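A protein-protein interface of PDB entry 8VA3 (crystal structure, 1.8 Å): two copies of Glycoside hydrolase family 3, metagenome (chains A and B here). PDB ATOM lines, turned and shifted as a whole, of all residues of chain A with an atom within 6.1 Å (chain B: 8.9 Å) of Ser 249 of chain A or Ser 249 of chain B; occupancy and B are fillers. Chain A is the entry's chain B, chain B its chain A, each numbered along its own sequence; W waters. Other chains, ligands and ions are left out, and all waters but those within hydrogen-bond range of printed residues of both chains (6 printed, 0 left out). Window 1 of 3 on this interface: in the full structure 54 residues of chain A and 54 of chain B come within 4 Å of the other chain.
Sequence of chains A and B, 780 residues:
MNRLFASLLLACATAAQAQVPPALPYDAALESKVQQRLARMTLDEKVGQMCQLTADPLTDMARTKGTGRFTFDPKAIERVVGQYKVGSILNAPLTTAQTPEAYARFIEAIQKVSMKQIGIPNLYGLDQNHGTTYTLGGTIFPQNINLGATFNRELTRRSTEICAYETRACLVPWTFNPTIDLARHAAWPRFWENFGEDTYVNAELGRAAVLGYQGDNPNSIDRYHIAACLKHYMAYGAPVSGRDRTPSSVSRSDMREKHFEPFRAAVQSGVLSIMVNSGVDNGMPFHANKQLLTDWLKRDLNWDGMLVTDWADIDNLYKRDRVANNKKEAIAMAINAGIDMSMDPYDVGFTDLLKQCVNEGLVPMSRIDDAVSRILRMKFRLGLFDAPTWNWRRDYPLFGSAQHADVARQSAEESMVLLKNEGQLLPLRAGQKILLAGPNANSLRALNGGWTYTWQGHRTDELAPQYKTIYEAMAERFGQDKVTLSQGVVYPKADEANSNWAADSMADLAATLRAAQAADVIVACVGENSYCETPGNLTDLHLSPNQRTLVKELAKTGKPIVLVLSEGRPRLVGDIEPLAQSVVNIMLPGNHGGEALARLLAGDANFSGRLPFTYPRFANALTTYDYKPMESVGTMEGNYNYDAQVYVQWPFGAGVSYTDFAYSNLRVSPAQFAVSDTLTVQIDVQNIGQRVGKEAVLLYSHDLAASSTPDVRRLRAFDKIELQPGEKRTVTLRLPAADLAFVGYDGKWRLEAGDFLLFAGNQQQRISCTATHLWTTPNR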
ATOM      1  N   ALA A 238     -27.084  13.346 -33.755  1.00  0.00           N
ATOM      2  CA  ALA A 238     -26.444  14.148 -32.709  1.00  0.00           C
ATOM      3  C   ALA A 238     -26.701  13.618 -31.298  1.00  0.00           C
ATOM      4  O   ALA A 238     -27.019  14.412 -30.407  1.00  0.00           O
ATOM      5  CB  ALA A 238     -26.930  15.602 -32.795  1.00  0.00           C
ATOM      6  N   PRO A 239     -26.600  12.314 -31.032  1.00  0.00           N
ATOM      7  CA  PRO A 239     -26.734  11.871 -29.642  1.00  0.00           C
ATOM      8  C   PRO A 239     -25.582  12.432 -28.840  1.00  0.00           C
ATOM      9  O   PRO A 239     -24.432  12.409 -29.288  1.00  0.00           O
ATOM     10  CB  PRO A 239     -26.651  10.340 -29.731  1.00  0.00           C
ATOM     11  CG  PRO A 239     -25.790  10.110 -30.965  1.00  0.00           C
ATOM     12  CD  PRO A 239     -26.168  11.215 -31.921  1.00  0.00           C
ATOM     13  N   VAL A 240     -25.909  12.954 -27.654  1.00  0.00           N
ATOM     14  CA  VAL A 240     -24.896  13.569 -26.791  1.00  0.00           C
ATOM     15  C   VAL A 240     -23.724  12.615 -26.570  1.00  0.00           C
ATOM     16  O   VAL A 240     -22.552  13.015 -26.611  1.00  0.00           O
ATOM     17  CB  VAL A 240     -25.538  13.981 -25.453  1.00  0.00           C
ATOM     18  CG1 VAL A 240     -24.474  14.379 -24.447  1.00  0.00           C
ATOM     19  CG2 VAL A 240     -26.542  15.133 -25.697  1.00  0.00           C
ATOM     20  N   PRO A 247     -30.350  10.197 -26.117  1.00  0.00           N
ATOM     21  CA  PRO A 247     -30.887  11.550 -26.357  1.00  0.00           C
ATOM     22  C   PRO A 247     -29.897  12.480 -27.051  1.00  0.00           C
ATOM     23  O   PRO A 247     -28.687  12.489 -26.770  1.00  0.00           O
ATOM     24  CB  PRO A 247     -31.219  12.067 -24.940  1.00  0.00           C
ATOM     25  CG  PRO A 247     -31.436  10.850 -24.125  1.00  0.00           C
ATOM     26  CD  PRO A 247     -30.447   9.820 -24.685  1.00  0.00           C
ATOM     27  N   SER A 248     -30.433  13.300 -27.938  1.00  0.00           N
ATOM     28  CA  SER A 248     -29.671  14.447 -28.383  1.00  0.00           C
ATOM     29  C   SER A 248     -30.046  15.619 -27.494  1.00  0.00           C
ATOM     30  O   SER A 248     -31.028  15.568 -26.741  1.00  0.00           O
ATOM     31  CB  SER A 248     -29.984  14.770 -29.851  1.00  0.00           C
ATOM     32  OG  SER A 248     -31.384  15.032 -30.016  1.00  0.00           O
ATOM     33  N   SER A 249     -29.288  16.713 -27.631  1.00  0.00           N
ATOM     34  CA  SER A 249     -29.550  17.944 -26.893  1.00  0.00           C
ATOM     35  C   SER A 249     -29.211  19.086 -27.848  1.00  0.00           C
ATOM     36  O   SER A 249     -28.193  19.766 -27.688  1.00  0.00           O
ATOM     37  CB  SER A 249     -28.730  18.025 -25.603  1.00  0.00           C
ATOM     38  OG  SER A 249     -29.112  19.142 -24.832  1.00  0.00           O
ATOM     39  N   VAL A 250     -30.069  19.254 -28.858  1.00  0.00           N
ATOM     40  CA  VAL A 250     -29.804  20.158 -29.973  1.00  0.00           C
ATOM     41  C   VAL A 250     -30.288  21.558 -29.614  1.00  0.00           C
ATOM     42  O   VAL A 250     -31.416  21.732 -29.124  1.00  0.00           O
ATOM     43  CB  VAL A 250     -30.491  19.657 -31.253  1.00  0.00           C
ATOM     44  CG1 VAL A 250     -30.335  20.687 -32.354  1.00  0.00           C
ATOM     45  CG2 VAL A 250     -29.900  18.313 -31.686  1.00  0.00           C
ATOM     46  N   SER A 251     -29.447  22.553 -29.878  1.00  0.00           N
ATOM     47  CA  SER A 251     -29.792  23.933 -29.570  1.00  0.00           C
ATOM     48  C   SER A 251     -30.877  24.436 -30.516  1.00  0.00           C
ATOM     49  O   SER A 251     -31.058  23.926 -31.623  1.00  0.00           O
ATOM     50  CB  SER A 251     -28.554  24.829 -29.663  1.00  0.00           C
ATOM     51  OG  SER A 251     -28.154  25.026 -31.015  1.00  0.00           O
ATOM     52  N   ASP A 254     -29.477  25.484 -33.920  1.00  0.00           N
ATOM     53  CA  ASP A 254     -28.989  24.323 -34.650  1.00  0.00           C
ATOM     54  C   ASP A 254     -30.139  23.483 -35.193  1.00  0.00           C
ATOM     55  O   ASP A 254     -30.031  22.930 -36.291  1.00  0.00           O
ATOM     56  CB  ASP A 254     -28.112  23.439 -33.753  1.00  0.00           C
ATOM     57  CG  ASP A 254     -26.676  23.959 -33.611  1.00  0.00           C
ATOM     58  OD1 ASP A 254     -26.313  24.907 -34.326  1.00  0.00           O
ATOM     59  OD2 ASP A 254     -25.911  23.409 -32.782  1.00  0.00           O
ATOM     60  N   VAL A 280     -34.794  10.651 -29.319  1.00  0.00           N
ATOM     61  CA  VAL A 280     -35.372  11.567 -28.344  1.00  0.00           C
ATOM     62  C   VAL A 280     -34.531  12.832 -28.335  1.00  0.00           C
ATOM     63  O   VAL A 280     -33.298  12.762 -28.430  1.00  0.00           O
ATOM     64  CB  VAL A 280     -35.389  10.915 -26.937  1.00  0.00           C
ATOM     65  CG1 VAL A 280     -35.536  11.986 -25.788  1.00  0.00           C
ATOM     66  CG2 VAL A 280     -36.479   9.816 -26.835  1.00  0.00           C
ATOM     67  N   ASP A 281     -35.189  13.994 -28.245  1.00  0.00           N
ATOM     68  CA  ASP A 281     -34.491  15.264 -28.001  1.00  0.00           C
ATOM     69  C   ASP A 281     -35.280  16.058 -26.964  1.00  0.00           C
ATOM     70  O   ASP A 281     -36.507  16.133 -27.057  1.00  0.00           O
ATOM     71  CB  ASP A 281     -34.332  16.092 -29.290  1.00  0.00           C
ATOM     72  CG  ASP A 281     -33.502  17.369 -29.060  1.00  0.00           C
ATOM     73  OD1 ASP A 281     -34.124  18.396 -28.701  1.00  0.00           O
ATOM     74  OD2 ASP A 281     -32.240  17.328 -29.207  1.00  0.00           O
ATOM     75  N   ASN A 282     -34.589  16.627 -25.976  1.00  0.00           N
ATOM     76  CA  ASN A 282     -35.247  17.420 -24.920  1.00  0.00           C
ATOM     77  C   ASN A 282     -36.380  16.608 -24.291  1.00  0.00           C
ATOM     78  O   ASN A 282     -37.469  17.110 -24.025  1.00  0.00           O
ATOM     79  CB  ASN A 282     -35.775  18.754 -25.468  1.00  0.00           C
ATOM     80  CG  ASN A 282     -36.327  19.683 -24.370  1.00  0.00           C
ATOM     81  OD1 ASN A 282     -35.791  19.745 -23.276  1.00  0.00           O
ATOM     82  ND2 ASN A 282     -37.408  20.374 -24.666  1.00  0.00           N
ATOM     83  N   ALA B 235     -25.171  27.039 -16.529  1.00  0.00           N
ATOM     84  CA  ALA B 235     -24.847  26.047 -17.553  1.00  0.00           C
ATOM     85  C   ALA B 235     -23.373  26.107 -17.974  1.00  0.00           C
ATOM     86  O   ALA B 235     -22.996  25.578 -19.041  1.00  0.00           O
ATOM     87  CB  ALA B 235     -25.774  26.200 -18.769  1.00  0.00           C
ATOM     88  N   GLY B 237     -20.857  24.503 -16.669  1.00  0.00           N
ATOM     89  CA  GLY B 237     -20.214  23.206 -16.565  1.00  0.00           C
ATOM     90  C   GLY B 237     -20.728  22.186 -17.559  1.00  0.00           C
ATOM     91  O   GLY B 237     -20.422  20.990 -17.457  1.00  0.00           O
ATOM     92  N   ALA B 238     -21.440  22.657 -18.577  1.00  0.00           N
ATOM     93  CA  ALA B 238     -21.907  21.713 -19.585  1.00  0.00           C
ATOM     94  C   ALA B 238     -21.389  22.020 -20.986  1.00  0.00           C
ATOM     95  O   ALA B 238     -22.162  21.940 -21.952  1.00  0.00           O
ATOM     96  CB  ALA B 238     -23.433  21.679 -19.603  1.00  0.00           C
ATOM     97  N   PRO B 239     -20.107  22.350 -21.169  1.00  0.00           N
ATOM     98  CA  PRO B 239     -19.624  22.524 -22.540  1.00  0.00           C
ATOM     99  C   PRO B 239     -19.738  21.207 -23.301  1.00  0.00           C
ATOM    100  O   PRO B 239     -19.374  20.146 -22.785  1.00  0.00           O
ATOM    101  CB  PRO B 239     -18.156  22.941 -22.361  1.00  0.00           C
ATOM    102  CG  PRO B 239     -17.724  22.270 -21.101  1.00  0.00           C
ATOM    103  CD  PRO B 239     -18.985  22.320 -20.199  1.00  0.00           C
ATOM    104  N   VAL B 240     -20.211  21.284 -24.543  1.00  0.00           N
ATOM    105  CA  VAL B 240     -20.396  20.064 -25.339  1.00  0.00           C
ATOM    106  C   VAL B 240     -19.120  19.233 -25.383  1.00  0.00           C
ATOM    107  O   VAL B 240     -19.151  18.011 -25.203  1.00  0.00           O
ATOM    108  CB  VAL B 240     -20.860  20.410 -26.765  1.00  0.00           C
ATOM    109  CG1 VAL B 240     -20.841  19.104 -27.659  1.00  0.00           C
ATOM    110  CG2 VAL B 240     -22.217  21.045 -26.699  1.00  0.00           C
ATOM    111  N   SER B 241     -17.983  19.876 -25.653  1.00  0.00           N
ATOM    112  CA  SER B 241     -16.728  19.157 -25.846  1.00  0.00           C
ATOM    113  C   SER B 241     -16.025  18.876 -24.535  1.00  0.00           C
ATOM    114  O   SER B 241     -15.010  18.170 -24.530  1.00  0.00           O
ATOM    115  CB  SER B 241     -15.767  19.961 -26.745  1.00  0.00           C
ATOM    116  OG  SER B 241     -15.364  21.164 -26.083  1.00  0.00           O
ATOM    117  N   THR B 246     -16.145  26.788 -23.940  1.00  0.00           N
ATOM    118  CA  THR B 246     -16.591  26.422 -25.272  1.00  0.00           C
ATOM    119  C   THR B 246     -18.092  26.168 -25.152  1.00  0.00           C
ATOM    120  O   THR B 246     -18.617  26.047 -24.040  1.00  0.00           O
ATOM    121  CB  THR B 246     -15.850  25.187 -25.834  1.00  0.00           C
ATOM    122  OG1 THR B 246     -16.117  24.036 -25.023  1.00  0.00           O
ATOM    123  CG2 THR B 246     -14.320  25.405 -25.854  1.00  0.00           C
ATOM    124  N   PRO B 247     -18.821  26.191 -26.269  1.00  0.00           N
ATOM    125  CA  PRO B 247     -20.288  26.273 -26.182  1.00  0.00           C
ATOM    126  C   PRO B 247     -20.908  25.087 -25.440  1.00  0.00           C
ATOM    127  O   PRO B 247     -20.491  23.940 -25.603  1.00  0.00           O
ATOM    128  CB  PRO B 247     -20.726  26.291 -27.651  1.00  0.00           C
ATOM    129  CG  PRO B 247     -19.510  26.969 -28.381  1.00  0.00           C
ATOM    130  CD  PRO B 247     -18.330  26.360 -27.660  1.00  0.00           C
ATOM    131  N   SER B 248     -21.908  25.389 -24.628  1.00  0.00           N
ATOM    132  CA  SER B 248     -22.875  24.387 -24.209  1.00  0.00           C
ATOM    133  C   SER B 248     -24.027  24.311 -25.210  1.00  0.00           C
ATOM    134  O   SER B 248     -24.222  25.189 -26.059  1.00  0.00           O
ATOM    135  CB  SER B 248     -23.398  24.707 -22.809  1.00  0.00           C
ATOM    136  OG  SER B 248     -24.043  25.981 -22.758  1.00  0.00           O
ATOM    137  N   SER B 249     -24.837  23.239 -25.088  1.00  0.00           N
ATOM    138  CA  SER B 249     -26.011  23.059 -25.934  1.00  0.00           C
ATOM    139  C   SER B 249     -27.097  22.431 -25.053  1.00  0.00           C
ATOM    140  O   SER B 249     -27.459  21.261 -25.208  1.00  0.00           O
ATOM    141  CB  SER B 249     -25.679  22.185 -27.151  1.00  0.00           C
ATOM    142  OG  SER B 249     -26.782  22.174 -28.019  1.00  0.00           O
ATOM    143  N   VAL B 250     -27.614  23.237 -24.075  1.00  0.00           N
ATOM    144  CA  VAL B 250     -28.475  22.700 -23.018  1.00  0.00           C
ATOM    145  C   VAL B 250     -29.917  22.698 -23.507  1.00  0.00           C
ATOM    146  O   VAL B 250     -30.377  23.673 -24.110  1.00  0.00           O
ATOM    147  CB  VAL B 250     -28.340  23.530 -21.724  1.00  0.00           C
ATOM    148  CG1 VAL B 250     -29.385  23.088 -20.688  1.00  0.00           C
ATOM    149  CG2 VAL B 250     -26.899  23.443 -21.148  1.00  0.00           C
ATOM    150  N   SER B 251     -30.625  21.593 -23.264  1.00  0.00           N
ATOM    151  CA  SER B 251     -32.002  21.482 -23.704  1.00  0.00           C
ATOM    152  C   SER B 251     -32.902  22.398 -22.880  1.00  0.00           C
ATOM    153  O   SER B 251     -32.579  22.782 -21.757  1.00  0.00           O
ATOM    154  CB  SER B 251     -32.487  20.031 -23.580  1.00  0.00           C
ATOM    155  OG  SER B 251     -32.702  19.713 -22.204  1.00  0.00           O
ATOM    156  N   ARG B 252     -34.054  22.736 -23.464  1.00  0.00           N
ATOM    157  CA  ARG B 252     -34.979  23.654 -22.808  1.00  0.00           C
ATOM    158  C   ARG B 252     -35.435  23.120 -21.449  1.00  0.00           C
ATOM    159  O   ARG B 252     -35.515  23.879 -20.488  1.00  0.00           O
ATOM    160  CB  ARG B 252     -36.179  23.924 -23.727  1.00  0.00           C
ATOM    161  CG  ARG B 252     -37.202  24.883 -23.153  1.00  0.00           C
ATOM    162  CD  ARG B 252     -38.223  25.370 -24.195  1.00  0.00           C
ATOM    163  NE  ARG B 252     -38.973  24.285 -24.817  1.00  0.00           N
ATOM    164  CZ  ARG B 252     -38.810  23.882 -26.075  1.00  0.00           C
ATOM    165  NH1 ARG B 252     -37.907  24.441 -26.863  1.00  0.00           N
ATOM    166  NH2 ARG B 252     -39.589  22.910 -26.558  1.00  0.00           N
ATOM    167  N   SER B 253     -35.720  21.815 -21.327  1.00  0.00           N
ATOM    168  CA  SER B 253     -36.103  21.323 -19.996  1.00  0.00           C
ATOM    169  C   SER B 253     -34.924  21.335 -19.013  1.00  0.00           C
ATOM    170  O   SER B 253     -35.103  21.735 -17.860  1.00  0.00           O
ATOM    171  CB  SER B 253     -36.740  19.939 -20.057  1.00  0.00           C
ATOM    172  OG  SER B 253     -38.032  20.013 -20.657  1.00  0.00           O
ATOM    173  N   ASP B 254     -33.710  20.953 -19.447  1.00  0.00           N
ATOM    174  CA  ASP B 254     -32.555  20.938 -18.541  1.00  0.00           C
ATOM    175  C   ASP B 254     -32.187  22.338 -18.040  1.00  0.00           C
ATOM    176  O   ASP B 254     -31.767  22.485 -16.889  1.00  0.00           O
ATOM    177  CB  ASP B 254     -31.298  20.312 -19.193  1.00  0.00           C
ATOM    178  CG  ASP B 254     -31.396  18.797 -19.371  1.00  0.00           C
ATOM    179  OD1 ASP B 254     -32.275  18.181 -18.781  1.00  0.00           O
ATOM    180  OD2 ASP B 254     -30.559  18.206 -20.090  1.00  0.00           O
ATOM    181  N   MET B 255     -32.296  23.371 -18.886  1.00  0.00           N
ATOM    182  CA  MET B 255     -31.907  24.715 -18.441  1.00  0.00           C
ATOM    183  C   MET B 255     -32.719  25.141 -17.211  1.00  0.00           C
ATOM    184  O   MET B 255     -32.175  25.663 -16.239  1.00  0.00           O
ATOM    185  CB  MET B 255     -32.100  25.716 -19.582  1.00  0.00           C
ATOM    186  CG  MET B 255     -31.476  27.115 -19.332  1.00  0.00           C
ATOM    187  SD  MET B 255     -29.663  27.064 -19.198  1.00  0.00           S
ATOM    188  CE  MET B 255     -29.216  27.147 -20.973  1.00  0.00           C
ATOM    189  N   HIS B 259     -30.104  23.327 -14.524  1.00  0.00           N
ATOM    190  CA  HIS B 259     -29.048  24.340 -14.401  1.00  0.00           C
ATOM    191  C   HIS B 259     -29.496  25.542 -13.574  1.00  0.00           C
ATOM    192  O   HIS B 259     -28.717  26.061 -12.757  1.00  0.00           O
ATOM    193  CB  HIS B 259     -28.574  24.755 -15.798  1.00  0.00           C
ATOM    194  CG  HIS B 259     -27.775  23.669 -16.464  1.00  0.00           C
ATOM    195  ND1 HIS B 259     -26.452  23.434 -16.147  1.00  0.00           N
ATOM    196  CD2 HIS B 259     -28.133  22.701 -17.341  1.00  0.00           C
ATOM    197  CE1 HIS B 259     -26.018  22.388 -16.841  1.00  0.00           C
ATOM    198  NE2 HIS B 259     -27.019  21.925 -17.570  1.00  0.00           N
ATOM    199  N   VAL B 280     -20.975  30.462 -23.487  1.00  0.00           N
ATOM    200  CA  VAL B 280     -21.953  30.627 -24.563  1.00  0.00           C
ATOM    201  C   VAL B 280     -22.869  29.403 -24.570  1.00  0.00           C
ATOM    202  O   VAL B 280     -22.405  28.265 -24.389  1.00  0.00           O
ATOM    203  CB  VAL B 280     -21.259  30.760 -25.953  1.00  0.00           C
ATOM    204  CG1 VAL B 280     -22.280  30.556 -27.098  1.00  0.00           C
ATOM    205  CG2 VAL B 280     -20.555  32.117 -26.118  1.00  0.00           C
ATOM    206  N   ASP B 281     -24.167  29.640 -24.811  1.00  0.00           N
ATOM    207  CA  ASP B 281     -25.132  28.586 -25.066  1.00  0.00           C
ATOM    208  C   ASP B 281     -26.016  29.039 -26.214  1.00  0.00           C
ATOM    209  O   ASP B 281     -26.406  30.209 -26.267  1.00  0.00           O
ATOM    210  CB  ASP B 281     -25.981  28.264 -23.815  1.00  0.00           C
ATOM    211  CG  ASP B 281     -26.949  27.105 -24.064  1.00  0.00           C
ATOM    212  OD1 ASP B 281     -28.074  27.371 -24.527  1.00  0.00           O
ATOM    213  OD2 ASP B 281     -26.576  25.938 -23.814  1.00  0.00           O
ATOM    214  N   ASN B 282     -26.271  28.128 -27.164  1.00  0.00           N
ATOM    215  CA  ASN B 282     -27.071  28.439 -28.348  1.00  0.00           C
ATOM    216  C   ASN B 282     -26.610  29.745 -29.003  1.00  0.00           C
ATOM    217  O   ASN B 282     -27.407  30.637 -29.338  1.00  0.00           O
ATOM    218  CB  ASN B 282     -28.565  28.475 -27.981  1.00  0.00           C
ATOM    219  CG  ASN B 282     -29.460  28.651 -29.200  1.00  0.00           C
ATOM    220  OD1 ASN B 282     -29.172  28.102 -30.270  1.00  0.00           O
ATOM    221  ND2 ASN B 282     -30.522  29.461 -29.060  1.00  0.00           N
ATOM    222  N   GLY B 283     -25.295  29.887 -29.142  1.00  0.00           N
ATOM    223  CA  GLY B 283     -24.752  31.027 -29.848  1.00  0.00           C
ATOM    224  C   GLY B 283     -24.749  32.312 -29.044  1.00  0.00           C
ATOM    225  O   GLY B 283     -24.194  33.306 -29.515  1.00  0.00           O
ATOM    226  N   PHE B 286     -23.617  34.447 -22.280  1.00  0.00           N
ATOM    227  CA  PHE B 286     -24.502  34.754 -21.140  1.00  0.00           C
ATOM    228  C   PHE B 286     -24.381  36.202 -20.718  1.00  0.00           C
ATOM    229  O   PHE B 286     -25.350  36.776 -20.217  1.00  0.00           O
ATOM    230  CB  PHE B 286     -24.215  33.835 -19.951  1.00  0.00           C
ATOM    231  CG  PHE B 286     -24.740  32.431 -20.185  1.00  0.00           C
ATOM    232  CD1 PHE B 286     -24.020  31.537 -20.977  1.00  0.00           C
ATOM    233  CD2 PHE B 286     -26.007  32.062 -19.699  1.00  0.00           C
ATOM    234  CE1 PHE B 286     -24.535  30.258 -21.248  1.00  0.00           C
ATOM    235  CE2 PHE B 286     -26.529  30.801 -19.940  1.00  0.00           C
ATOM    236  CZ  PHE B 286     -25.807  29.883 -20.713  1.00  0.00           C
HETATM  237  O   HOH W   1     -26.437  27.551 -31.719  1.00  0.00           O
HETATM  238  O   HOH W   2     -26.784  21.683 -30.872  1.00  0.00           O
HETATM  239  O   HOH W   3     -29.175  19.573 -21.971  1.00  0.00           O
HETATM  240  O   HOH W   4     -36.748  21.591 -27.265  1.00  0.00           O
HETATM  241  O   HOH W   5     -39.080  17.871 -22.047  1.00  0.00           O
HETATM  242  O   HOH W   6     -38.647  22.023 -22.374  1.00  0.00           O
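The backbone NH (N) of Arg 252 of chain B sits at hydrogen-bond distance from the side-chain amide oxygen (OD1) of Asn 282 of chain A (3.5 Å). OG of Ser 249 of chain A is in hydrogen-bond range of N of Ser 251 of chain B (3.3 Å). O of Ser 249 of chain B lies within hydrogen-bond range of OG of Ser 249 of chain A (2.7 Å). The side-chain hydroxyl (OG) of Ser 251 of chain B sits at hydrogen-bond distance from the side-chain amide oxygen (OD1) of Asn 282 of chain A. The side-chain hydroxyl (OG) of Ser 251 of chain A sits at hydrogen-bond distance from the side-chain amide oxygen (OD1) of Asn 282 of chain B (3.3 Å). The side-chain hydroxyl (OG) of Ser 249 of chain B is in hydrogen-bond range of the backbone NH (N) of Ser 251 of chain A (3.3 Å). N of Ser 253 of chain B lies within hydrogen-bond range of OD1 of Asn 282 of chain A, 2.8 Å away.
The backbone NH of Val 250 of chain A lies within hydrogen-bond range of the side-chain carboxylate of Asp 281 of chain A, at 2.9 Å. The backbone NH (N) of Ser 249 of chain B sits at hydrogen-bond distance from the side-chain carboxylate (OD2) of Asp 281 of chain B, at 3.5 Å. The side-chain carboxylate of Asp 281 of chain A sits at hydrogen-bond distance from the backbone NH of Ser 249 of chain A (3.4 Å). N of Asp 254 of chain B lies within hydrogen-bond range of OG of Ser 251 of chain B (3.2 Å). The backbone NH (N) of Val 250 of chain B is in hydrogen-bond range of the side-chain carboxylate (OD2) of Asp 281 of chain B (2.9 Å). OG of Ser 251 of chain A sits close to N of Asp 254 of chain A, 3.2 Å away.
Among the printed residues, pairs that only touch across the chains: Ser 249 of chain A with Val 250 of chain B and Val 250 of chain A with Ser 249 of chain B.
Of the printed residues of chain B, Ser 249 of chain A touches Ser 249 (2.7 Å), Val 250 (3.9 Å) and Ser 251 (3.3 Å). Ser 249 of chain B touches three residues of chain A. No residue of chain B comes within 4 Å of Ser 248 of chain A. Printed residues of chain B within 4 Å of Val 250 of chain A: Ser 249 (3.9 Å). Printed residues of chain A within 4 Å of Ser 253 of chain B: Asn 282. Printed residues of chain A within 4 Å of Val 250 of chain B: Ser 249 (3.9 Å). Of the printed residues of chain B, Asn 282 of chain A touches Ser 251 (3.3 Å), Arg 252 (3.5 Å) and Ser 253 (2.8 Å). The nearest printed residue of chain A that does not touch Val 250 of chain B is Val 250 of chain A (5.5 Å).
Of the 12 printed residues of chain A, 4 touch a printed residue of chain B. Printed residues of chain A that touch a printed residue of chain B: Ser 249, Val 250, Ser 251 and Asn 282. Among the printed residues, 9 pairs touch across the chains.
Ser 249 of chain A touches its own counterpart, Ser 249 of chain B. Ser 249 of chain A touches Val 250 of chain B, and with the chains exchanged Val 250 of chain A touches Ser 249 of chain B. Ser 249 of chain A touches Ser 251 of chain B, and with the chains exchanged Ser 251 of chain A touches Ser 249 of chain B. Ser 251 of chain A touches Asn 282 of chain B, and with the chains exchanged Asn 282 of chain A touches Ser 251 of chain B. Positions printed for both chains: 238, 239, 240, 247, 248, 249, 250, 251, 254, 280, 281 and 282.
Water W5 lies within hydrogen-bond range of the backbone carbonyl oxygen of Asn 282 of chain A (2.7 Å) and the side-chain hydroxyl of Ser 253 of chain B (2.8 Å). Water W3 lies within hydrogen-bond range of OD2 of Asp 254 of chain B (2.7 Å), N of Ser 251 of chain B (2.8 Å) and OG of Ser 249 of chain A (2.9 Å). Water W6 lies within hydrogen-bond range of the side-chain hydroxyl of Ser 253 of chain B, the side-chain amide nitrogen of Asn 282 of chain A and the guanidinium group of Arg 252 of chain B. Water W2 lies within hydrogen-bond range of the side-chain carboxylate of Asp 254 of chain A, the side-chain hydroxyl of Ser 249 of chain B and the backbone NH of Ser 251 of chain A. Water W4 lies within hydrogen-bond range of the side-chain amide nitrogen (ND2) of Asn 282 of chain A (2.9 Å) and the guanidinium group (NH1) of Arg 252 of chain B (3.1 Å). Water W1 bridges OG of Ser 251 of chain A and OD1 of Asn 282 of chain B.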
